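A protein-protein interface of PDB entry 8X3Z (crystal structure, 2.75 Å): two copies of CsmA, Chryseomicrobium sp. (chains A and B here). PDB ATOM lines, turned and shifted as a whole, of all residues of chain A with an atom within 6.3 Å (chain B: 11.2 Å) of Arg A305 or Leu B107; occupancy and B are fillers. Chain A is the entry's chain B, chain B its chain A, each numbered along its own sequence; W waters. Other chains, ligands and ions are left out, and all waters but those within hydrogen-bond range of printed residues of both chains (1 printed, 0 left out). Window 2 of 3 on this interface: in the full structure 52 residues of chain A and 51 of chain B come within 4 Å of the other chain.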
ATOM      1  N   SER A 274       5.751 -25.279  34.635  1.00  0.00           N
ATOM      2  CA  SER A 274       4.608 -25.552  33.761  1.00  0.00           C
ATOM      3  C   SER A 274       4.727 -24.859  32.410  1.00  0.00           C
ATOM      4  O   SER A 274       3.883 -25.078  31.530  1.00  0.00           O
ATOM      5  CB  SER A 274       3.290 -25.120  34.409  1.00  0.00           C
ATOM      6  OG  SER A 274       3.365 -23.776  34.811  1.00  0.00           O
ATOM      7  N   LEU A 275       5.764 -24.048  32.219  1.00  0.00           N
ATOM      8  CA  LEU A 275       5.992 -23.419  30.941  1.00  0.00           C
ATOM      9  C   LEU A 275       4.843 -22.480  30.587  1.00  0.00           C
ATOM     10  O   LEU A 275       4.364 -22.447  29.451  1.00  0.00           O
ATOM     11  CB  LEU A 275       6.221 -24.488  29.876  1.00  0.00           C
ATOM     12  CG  LEU A 275       7.474 -25.329  30.166  1.00  0.00           C
ATOM     13  CD1 LEU A 275       7.667 -26.363  29.038  1.00  0.00           C
ATOM     14  CD2 LEU A 275       8.720 -24.450  30.344  1.00  0.00           C
ATOM     15  N   GLY A 276       4.423 -21.704  31.587  1.00  0.00           N
ATOM     16  CA  GLY A 276       3.396 -20.700  31.436  1.00  0.00           C
ATOM     17  C   GLY A 276       3.961 -19.367  30.996  1.00  0.00           C
ATOM     18  O   GLY A 276       5.155 -19.224  30.718  1.00  0.00           O
ATOM     19  N   GLU A 277       3.068 -18.365  30.960  1.00  0.00           N
ATOM     20  CA  GLU A 277       3.369 -17.088  30.317  1.00  0.00           C
ATOM     21  C   GLU A 277       4.656 -16.443  30.829  1.00  0.00           C
ATOM     22  O   GLU A 277       5.489 -15.993  30.031  1.00  0.00           O
ATOM     23  CB  GLU A 277       2.200 -16.127  30.484  1.00  0.00           C
ATOM     24  CG  GLU A 277       2.222 -14.997  29.494  1.00  0.00           C
ATOM     25  CD  GLU A 277       1.169 -13.955  29.789  1.00  0.00           C
ATOM     26  OE1 GLU A 277       1.412 -12.774  29.469  1.00  0.00           O
ATOM     27  OE2 GLU A 277       0.099 -14.308  30.338  1.00  0.00           O
ATOM     28  N   TYR A 283       5.367 -17.356  25.739  1.00  0.00           N
ATOM     29  CA  TYR A 283       5.355 -18.528  24.850  1.00  0.00           C
ATOM     30  C   TYR A 283       6.288 -18.351  23.658  1.00  0.00           C
ATOM     31  O   TYR A 283       5.935 -18.594  22.502  1.00  0.00           O
ATOM     32  CB  TYR A 283       3.920 -18.871  24.425  1.00  0.00           C
ATOM     33  CG  TYR A 283       3.021 -19.000  25.648  1.00  0.00           C
ATOM     34  CD1 TYR A 283       3.103 -20.112  26.484  1.00  0.00           C
ATOM     35  CD2 TYR A 283       2.141 -17.977  25.997  1.00  0.00           C
ATOM     36  CE1 TYR A 283       2.310 -20.210  27.619  1.00  0.00           C
ATOM     37  CE2 TYR A 283       1.349 -18.062  27.132  1.00  0.00           C
ATOM     38  CZ  TYR A 283       1.435 -19.182  27.938  1.00  0.00           C
ATOM     39  OH  TYR A 283       0.650 -19.275  29.065  1.00  0.00           O
ATOM     40  N   ASP A 299       2.868 -33.328  37.695  1.00  0.00           N
ATOM     41  CA  ASP A 299       1.532 -33.099  37.176  1.00  0.00           C
ATOM     42  C   ASP A 299       1.471 -33.540  35.712  1.00  0.00           C
ATOM     43  O   ASP A 299       2.037 -32.886  34.843  1.00  0.00           O
ATOM     44  CB  ASP A 299       1.206 -31.620  37.338  1.00  0.00           C
ATOM     45  CG  ASP A 299      -0.188 -31.252  36.807  1.00  0.00           C
ATOM     46  OD1 ASP A 299      -0.929 -32.153  36.361  1.00  0.00           O
ATOM     47  OD2 ASP A 299      -0.522 -30.051  36.818  1.00  0.00           O
ATOM     48  N   SER A 301      -0.714 -33.383  33.507  1.00  0.00           N
ATOM     49  CA  SER A 301      -1.326 -32.467  32.557  1.00  0.00           C
ATOM     50  C   SER A 301      -0.351 -31.475  31.901  1.00  0.00           C
ATOM     51  O   SER A 301      -0.749 -30.865  30.902  1.00  0.00           O
ATOM     52  CB  SER A 301      -2.474 -31.719  33.274  1.00  0.00           C
ATOM     53  OG  SER A 301      -2.108 -31.053  34.436  1.00  0.00           O
ATOM     54  N   VAL A 302       0.851 -31.239  32.456  1.00  0.00           N
ATOM     55  CA  VAL A 302       1.685 -30.148  31.942  1.00  0.00           C
ATOM     56  C   VAL A 302       2.441 -30.537  30.676  1.00  0.00           C
ATOM     57  O   VAL A 302       2.869 -29.659  29.922  1.00  0.00           O
ATOM     58  CB  VAL A 302       2.695 -29.602  32.968  1.00  0.00           C
ATOM     59  CG1 VAL A 302       2.029 -29.186  34.217  1.00  0.00           C
ATOM     60  CG2 VAL A 302       3.822 -30.587  33.292  1.00  0.00           C
ATOM     61  N   PHE A 303       2.656 -31.814  30.431  1.00  0.00           N
ATOM     62  CA  PHE A 303       3.444 -32.210  29.274  1.00  0.00           C
ATOM     63  C   PHE A 303       2.666 -31.987  27.986  1.00  0.00           C
ATOM     64  O   PHE A 303       1.517 -32.418  27.863  1.00  0.00           O
ATOM     65  CB  PHE A 303       3.836 -33.680  29.387  1.00  0.00           C
ATOM     66  CG  PHE A 303       4.557 -34.032  30.661  1.00  0.00           C
ATOM     67  CD1 PHE A 303       5.784 -33.461  30.963  1.00  0.00           C
ATOM     68  CD2 PHE A 303       4.001 -34.927  31.559  1.00  0.00           C
ATOM     69  CE1 PHE A 303       6.455 -33.790  32.120  1.00  0.00           C
ATOM     70  CE2 PHE A 303       4.672 -35.253  32.723  1.00  0.00           C
ATOM     71  CZ  PHE A 303       5.899 -34.687  33.001  1.00  0.00           C
ATOM     72  N   ASN A 304       3.308 -31.329  27.023  1.00  0.00           N
ATOM     73  CA  ASN A 304       2.796 -31.110  25.668  1.00  0.00           C
ATOM     74  C   ASN A 304       1.616 -30.136  25.598  1.00  0.00           C
ATOM     75  O   ASN A 304       0.903 -30.088  24.577  1.00  0.00           O
ATOM     76  CB  ASN A 304       2.431 -32.440  25.005  1.00  0.00           C
ATOM     77  CG  ASN A 304       3.607 -33.391  24.954  1.00  0.00           C
ATOM     78  OD1 ASN A 304       4.712 -33.021  24.553  1.00  0.00           O
ATOM     79  ND2 ASN A 304       3.386 -34.616  25.396  1.00  0.00           N
ATOM     80  N   ARG A 305       1.411 -29.317  26.636  1.00  0.00           N
ATOM     81  CA  ARG A 305       0.416 -28.255  26.527  1.00  0.00           C
ATOM     82  C   ARG A 305       0.756 -27.351  25.351  1.00  0.00           C
ATOM     83  O   ARG A 305      -0.072 -27.115  24.471  1.00  0.00           O
ATOM     84  CB  ARG A 305       0.360 -27.443  27.817  1.00  0.00           C
ATOM     85  CG  ARG A 305      -0.481 -28.004  28.930  1.00  0.00           C
ATOM     86  CD  ARG A 305      -0.357 -27.142  30.217  1.00  0.00           C
ATOM     87  NE  ARG A 305      -0.944 -27.840  31.362  1.00  0.00           N
ATOM     88  CZ  ARG A 305      -1.032 -27.351  32.592  1.00  0.00           C
ATOM     89  NH1 ARG A 305      -0.572 -26.142  32.888  1.00  0.00           N
ATOM     90  NH2 ARG A 305      -1.593 -28.081  33.534  1.00  0.00           N
ATOM     91  N   LYS A 306       1.973 -26.894  25.286  1.00  0.00           N
ATOM     92  CA  LYS A 306       2.398 -26.031  24.194  1.00  0.00           C
ATOM     93  C   LYS A 306       3.745 -26.462  23.621  1.00  0.00           C
ATOM     94  O   LYS A 306       3.906 -26.490  22.396  1.00  0.00           O
ATOM     95  CB  LYS A 306       2.453 -24.551  24.677  1.00  0.00           C
ATOM     96  CG  LYS A 306       3.028 -23.584  23.663  1.00  0.00           C
ATOM     97  CD  LYS A 306       1.998 -23.200  22.627  1.00  0.00           C
ATOM     98  CE  LYS A 306       2.582 -22.403  21.499  1.00  0.00           C
ATOM     99  NZ  LYS A 306       1.480 -22.052  20.568  1.00  0.00           N
ATOM    100  N   TYR A 307       4.692 -26.893  24.462  1.00  0.00           N
ATOM    101  CA  TYR A 307       6.015 -27.312  24.007  1.00  0.00           C
ATOM    102  C   TYR A 307       6.073 -28.833  23.882  1.00  0.00           C
ATOM    103  O   TYR A 307       5.940 -29.551  24.881  1.00  0.00           O
ATOM    104  CB  TYR A 307       7.096 -26.815  24.973  1.00  0.00           C
ATOM    105  CG  TYR A 307       7.190 -25.311  25.036  1.00  0.00           C
ATOM    106  CD1 TYR A 307       6.302 -24.566  25.814  1.00  0.00           C
ATOM    107  CD2 TYR A 307       8.153 -24.616  24.296  1.00  0.00           C
ATOM    108  CE1 TYR A 307       6.377 -23.170  25.867  1.00  0.00           C
ATOM    109  CE2 TYR A 307       8.240 -23.210  24.355  1.00  0.00           C
ATOM    110  CZ  TYR A 307       7.350 -22.498  25.132  1.00  0.00           C
ATOM    111  OH  TYR A 307       7.434 -21.116  25.180  1.00  0.00           O
ATOM    112  N   VAL B 100      -7.900 -14.201  30.169  1.00  0.00           N
ATOM    113  CA  VAL B 100      -6.693 -14.355  29.355  1.00  0.00           C
ATOM    114  C   VAL B 100      -7.130 -14.688  27.931  1.00  0.00           C
ATOM    115  O   VAL B 100      -8.289 -15.095  27.719  1.00  0.00           O
ATOM    116  CB  VAL B 100      -5.738 -15.423  29.925  1.00  0.00           C
ATOM    117  CG1 VAL B 100      -5.293 -15.035  31.346  1.00  0.00           C
ATOM    118  CG2 VAL B 100      -6.370 -16.865  29.853  1.00  0.00           C
ATOM    119  N   PRO B 101      -6.245 -14.547  26.935  1.00  0.00           N
ATOM    120  CA  PRO B 101      -6.665 -14.758  25.542  1.00  0.00           C
ATOM    121  C   PRO B 101      -7.236 -16.153  25.311  1.00  0.00           C
ATOM    122  O   PRO B 101      -6.834 -17.132  25.934  1.00  0.00           O
ATOM    123  CB  PRO B 101      -5.372 -14.541  24.745  1.00  0.00           C
ATOM    124  CG  PRO B 101      -4.599 -13.555  25.571  1.00  0.00           C
ATOM    125  CD  PRO B 101      -4.902 -13.939  27.017  1.00  0.00           C
ATOM    126  N   VAL B 102      -8.232 -16.215  24.430  1.00  0.00           N
ATOM    127  CA  VAL B 102      -8.802 -17.497  24.035  1.00  0.00           C
ATOM    128  C   VAL B 102      -7.709 -18.506  23.715  1.00  0.00           C
ATOM    129  O   VAL B 102      -7.762 -19.651  24.178  1.00  0.00           O
ATOM    130  CB  VAL B 102      -9.760 -17.302  22.855  1.00  0.00           C
ATOM    131  CG1 VAL B 102     -10.598 -18.539  22.699  1.00  0.00           C
ATOM    132  CG2 VAL B 102     -10.620 -16.071  23.126  1.00  0.00           C
ATOM    133  N   SER B 103      -6.750 -18.116  22.850  1.00  0.00           N
ATOM    134  CA  SER B 103      -5.639 -18.999  22.451  1.00  0.00           C
ATOM    135  C   SER B 103      -4.861 -19.588  23.644  1.00  0.00           C
ATOM    136  O   SER B 103      -4.432 -20.755  23.601  1.00  0.00           O
ATOM    137  CB  SER B 103      -4.686 -18.266  21.488  1.00  0.00           C
ATOM    138  OG  SER B 103      -4.004 -17.169  22.092  1.00  0.00           O
ATOM    139  N   THR B 104      -4.644 -18.803  24.706  1.00  0.00           N
ATOM    140  CA  THR B 104      -3.716 -19.192  25.771  1.00  0.00           C
ATOM    141  C   THR B 104      -4.399 -19.706  27.043  1.00  0.00           C
ATOM    142  O   THR B 104      -3.713 -19.940  28.044  1.00  0.00           O
ATOM    143  CB  THR B 104      -2.786 -18.027  26.134  1.00  0.00           C
ATOM    144  OG1 THR B 104      -3.521 -17.023  26.850  1.00  0.00           O
ATOM    145  CG2 THR B 104      -2.137 -17.432  24.896  1.00  0.00           C
ATOM    146  N   LEU B 105      -5.719 -19.887  27.052  1.00  0.00           N
ATOM    147  CA  LEU B 105      -6.339 -20.492  28.218  1.00  0.00           C
ATOM    148  C   LEU B 105      -6.045 -21.985  28.180  1.00  0.00           C
ATOM    149  O   LEU B 105      -6.150 -22.623  27.117  1.00  0.00           O
ATOM    150  CB  LEU B 105      -7.837 -20.204  28.297  1.00  0.00           C
ATOM    151  CG  LEU B 105      -8.500 -20.700  29.613  1.00  0.00           C
ATOM    152  CD1 LEU B 105      -8.415 -19.699  30.790  1.00  0.00           C
ATOM    153  CD2 LEU B 105      -9.936 -21.123  29.445  1.00  0.00           C
ATOM    154  N   GLY B 106      -5.657 -22.548  29.332  1.00  0.00           N
ATOM    155  CA  GLY B 106      -5.089 -23.870  29.434  1.00  0.00           C
ATOM    156  C   GLY B 106      -3.571 -23.907  29.538  1.00  0.00           C
ATOM    157  O   GLY B 106      -3.016 -24.961  29.873  1.00  0.00           O
ATOM    158  N   LEU B 107      -2.888 -22.787  29.286  1.00  0.00           N
ATOM    159  CA  LEU B 107      -1.434 -22.738  29.234  1.00  0.00           C
ATOM    160  C   LEU B 107      -0.824 -22.052  30.451  1.00  0.00           C
ATOM    161  O   LEU B 107       0.370 -21.721  30.433  1.00  0.00           O
ATOM    162  CB  LEU B 107      -0.975 -22.028  27.963  1.00  0.00           C
ATOM    163  CG  LEU B 107      -1.409 -22.750  26.689  1.00  0.00           C
ATOM    164  CD1 LEU B 107      -0.755 -22.099  25.461  1.00  0.00           C
ATOM    165  CD2 LEU B 107      -1.073 -24.241  26.791  1.00  0.00           C
ATOM    166  N   ASN B 108      -1.603 -21.827  31.506  1.00  0.00           N
ATOM    167  CA  ASN B 108      -1.133 -21.101  32.686  1.00  0.00           C
ATOM    168  C   ASN B 108      -0.593 -19.725  32.278  1.00  0.00           C
ATOM    169  O   ASN B 108       0.535 -19.326  32.604  1.00  0.00           O
ATOM    170  CB  ASN B 108      -0.088 -21.914  33.477  1.00  0.00           C
ATOM    171  CG  ASN B 108      -0.715 -23.031  34.331  1.00  0.00           C
ATOM    172  OD1 ASN B 108      -1.947 -23.189  34.378  1.00  0.00           O
ATOM    173  ND2 ASN B 108       0.135 -23.811  35.004  1.00  0.00           N
ATOM    174  N   ALA B 109      -1.451 -18.990  31.572  1.00  0.00           N
ATOM    175  CA  ALA B 109      -1.241 -17.579  31.300  1.00  0.00           C
ATOM    176  C   ALA B 109      -1.333 -16.784  32.604  1.00  0.00           C
ATOM    177  O   ALA B 109      -1.898 -17.236  33.607  1.00  0.00           O
ATOM    178  CB  ALA B 109      -2.292 -17.088  30.302  1.00  0.00           C
ATOM    179  N   SER B 110      -0.807 -15.568  32.593  1.00  0.00           N
ATOM    180  CA  SER B 110      -0.755 -14.828  33.843  1.00  0.00           C
ATOM    181  C   SER B 110      -2.166 -14.423  34.274  1.00  0.00           C
ATOM    182  O   SER B 110      -2.932 -13.830  33.494  1.00  0.00           O
ATOM    183  CB  SER B 110       0.139 -13.612  33.688  1.00  0.00           C
ATOM    184  OG  SER B 110       0.567 -13.109  34.953  1.00  0.00           O
ATOM    185  N   GLN B 111      -2.515 -14.726  35.526  1.00  0.00           N
ATOM    186  CA  GLN B 111      -3.871 -14.490  36.056  1.00  0.00           C
ATOM    187  C   GLN B 111      -4.943 -15.316  35.324  1.00  0.00           C
ATOM    188  O   GLN B 111      -6.102 -14.911  35.217  1.00  0.00           O
ATOM    189  CB  GLN B 111      -4.204 -12.994  36.012  1.00  0.00           C
ATOM    190  CG  GLN B 111      -3.159 -12.157  36.737  1.00  0.00           C
ATOM    191  CD  GLN B 111      -3.551 -10.702  36.854  1.00  0.00           C
ATOM    192  OE1 GLN B 111      -3.357 -10.082  37.898  1.00  0.00           O
ATOM    193  NE2 GLN B 111      -4.099 -10.143  35.776  1.00  0.00           N
ATOM    194  N   GLU B 112      -4.599 -16.522  34.872  1.00  0.00           N
ATOM    195  CA  GLU B 112      -5.572 -17.386  34.217  1.00  0.00           C
ATOM    196  C   GLU B 112      -6.581 -17.935  35.232  1.00  0.00           C
ATOM    197  O   GLU B 112      -6.209 -18.406  36.313  1.00  0.00           O
ATOM    198  CB  GLU B 112      -4.845 -18.527  33.497  1.00  0.00           C
ATOM    199  CG  GLU B 112      -5.726 -19.692  33.027  1.00  0.00           C
ATOM    200  CD  GLU B 112      -5.014 -20.623  32.038  1.00  0.00           C
ATOM    201  OE1 GLU B 112      -5.427 -21.796  31.925  1.00  0.00           O
ATOM    202  OE2 GLU B 112      -4.055 -20.186  31.362  1.00  0.00           O
ATOM    203  N   LEU B 113      -7.866 -17.793  34.920  1.00  0.00           N
ATOM    204  CA  LEU B 113      -8.900 -18.490  35.674  1.00  0.00           C
ATOM    205  C   LEU B 113     -10.237 -18.401  34.960  1.00  0.00           C
ATOM    206  O   LEU B 113     -10.678 -17.304  34.603  1.00  0.00           O
ATOM    207  CB  LEU B 113      -9.005 -17.926  37.080  1.00  0.00           C
ATOM    208  CG  LEU B 113     -10.059 -18.668  37.880  1.00  0.00           C
ATOM    209  CD1 LEU B 113      -9.547 -20.051  38.191  1.00  0.00           C
ATOM    210  CD2 LEU B 113     -10.341 -17.915  39.160  1.00  0.00           C
ATOM    211  N   ASP B 114     -10.891 -19.534  34.719  1.00  0.00           N
ATOM    212  CA  ASP B 114     -12.176 -19.505  34.037  1.00  0.00           C
ATOM    213  C   ASP B 114     -13.238 -19.156  35.065  1.00  0.00           C
ATOM    214  O   ASP B 114     -13.554 -19.976  35.945  1.00  0.00           O
ATOM    215  CB  ASP B 114     -12.446 -20.836  33.334  1.00  0.00           C
ATOM    216  CG  ASP B 114     -13.734 -20.811  32.459  1.00  0.00           C
ATOM    217  OD1 ASP B 114     -14.181 -19.708  32.037  1.00  0.00           O
ATOM    218  OD2 ASP B 114     -14.293 -21.906  32.174  1.00  0.00           O
HETATM  219  O   HOH W   1       1.515 -24.337  30.989  1.00  0.00           O
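The backbone carbonyl oxygen of Leu B107 sits at hydrogen-bond distance from the side-chain hydroxyl of Tyr A283. The side-chain hydroxyl (OG) of Ser A274 sits at hydrogen-bond distance from the side-chain amide nitrogen (ND2) of Asn B108. The backbone carbonyl oxygen (O) of Asn B108 sits at hydrogen-bond distance from the backbone NH (N) of Glu A277, at 3.2 Å. The side-chain amide nitrogen (ND2) of Asn B108 lies close to the guanidinium group (NH1) of Arg A305, at 3.2 Å. OH of Tyr A283 lies within hydrogen-bond range of N of Ala B109, 3.3 Å away. The side-chain carboxylate (OE2) of Glu A277 is in hydrogen-bond range of the backbone NH (N) of Ser B110 (2.7 Å).
Of chain B, only Asn B108 comes within 4 Å of Ser A274. Gly A276 touches just these residues of chain B: Leu B107 (3.3 Å) and Asn B108 (3.4 Å). Of the printed residues of chain B, Glu A277 touches Asn B108, Ala B109 and Ser B110. No residue of chain B comes within 4 Å of Ser A301. Arg A305 touches just these residues of chain B: Gly B106, Leu B107 and Asn B108. Leu B107 touches just these residues of chain A: Gly A276 (3.3 Å), Tyr A283 (2.8 Å) and Arg A305 (3.7 Å). Printed residues of chain A within 4 Å of Asn B108: Ser A274 (3.2 Å), Gly A276 (3.4 Å), Glu A277 (3.2 Å), Tyr A283 (3.5 Å) and Arg A305 (3.2 Å). Asp B114 touches none of the printed residues of chain A. The nearest residue of chain B that does not touch Arg A305 is Glu B112 (6.6 Å). The nearest residue of chain A that does not touch Leu B107 is Lys A306 (4.1 Å).
Hydrophobic or aromatic side chains of chain B that line the printed part of chain A: Leu B107 and Ala B109. Printed residues of chain A that touch a printed residue of chain B: Ser A274, Gly A276, Glu A277, Tyr A283 and Arg A305. Hydrophobic or aromatic side chains of chain A that line the printed part of chain B: Tyr A283. Among the printed residues, 12 pairs touch across the chains. Among the printed residues, no Asp or Glu carboxylate lies within 4 Å of a Lys or Arg side-chain nitrogen of the other chain.
No position is printed for both chains. Of the 12 pairs that touch across the chains among the printed residues, none has its exchanged pair printed and touching as well.
The side-chain carboxylate (OE1) of Glu B112 sits at hydrogen-bond distance from the backbone NH (N) of Gly B106, at 2.7 Å. The backbone NH (N) of Asn B108 lies within hydrogen-bond range of the side-chain carboxylate (OE2) of Glu B112 (3.0 Å). The side-chain carboxylate (OE2) of Glu B112 lies within hydrogen-bond range of the backbone NH (N) of Ala B109. N of Glu A277 is in hydrogen-bond range of OH of Tyr A283, 3.2 Å away. The guanidinium group of Arg A305 is in salt-bridge range of the side-chain carboxylate of Asp A299, at 3.98 Å. The backbone carbonyl oxygen (O) of Ser A301 is in hydrogen-bond range of the guanidinium group (NE) of Arg A305, 3.1 Å away.
Among the printed residues, merely in contact across the chains: Gly A276 with Leu B107 (3.3 Å), Gly A276 with Asn B108 (3.4 Å), Arg A305 with Gly B106 (3.5 Å), Tyr A283 with Asn B108 (3.5 Å), Glu A277 with Ala B109 (3.6 Å) and Arg A305 with Leu B107 (3.7 Å).
Water W1 lies within hydrogen-bond range of the backbone carbonyl oxygen of Ser A274, the backbone carbonyl oxygen of Leu B107 and the guanidinium group of Arg A305.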
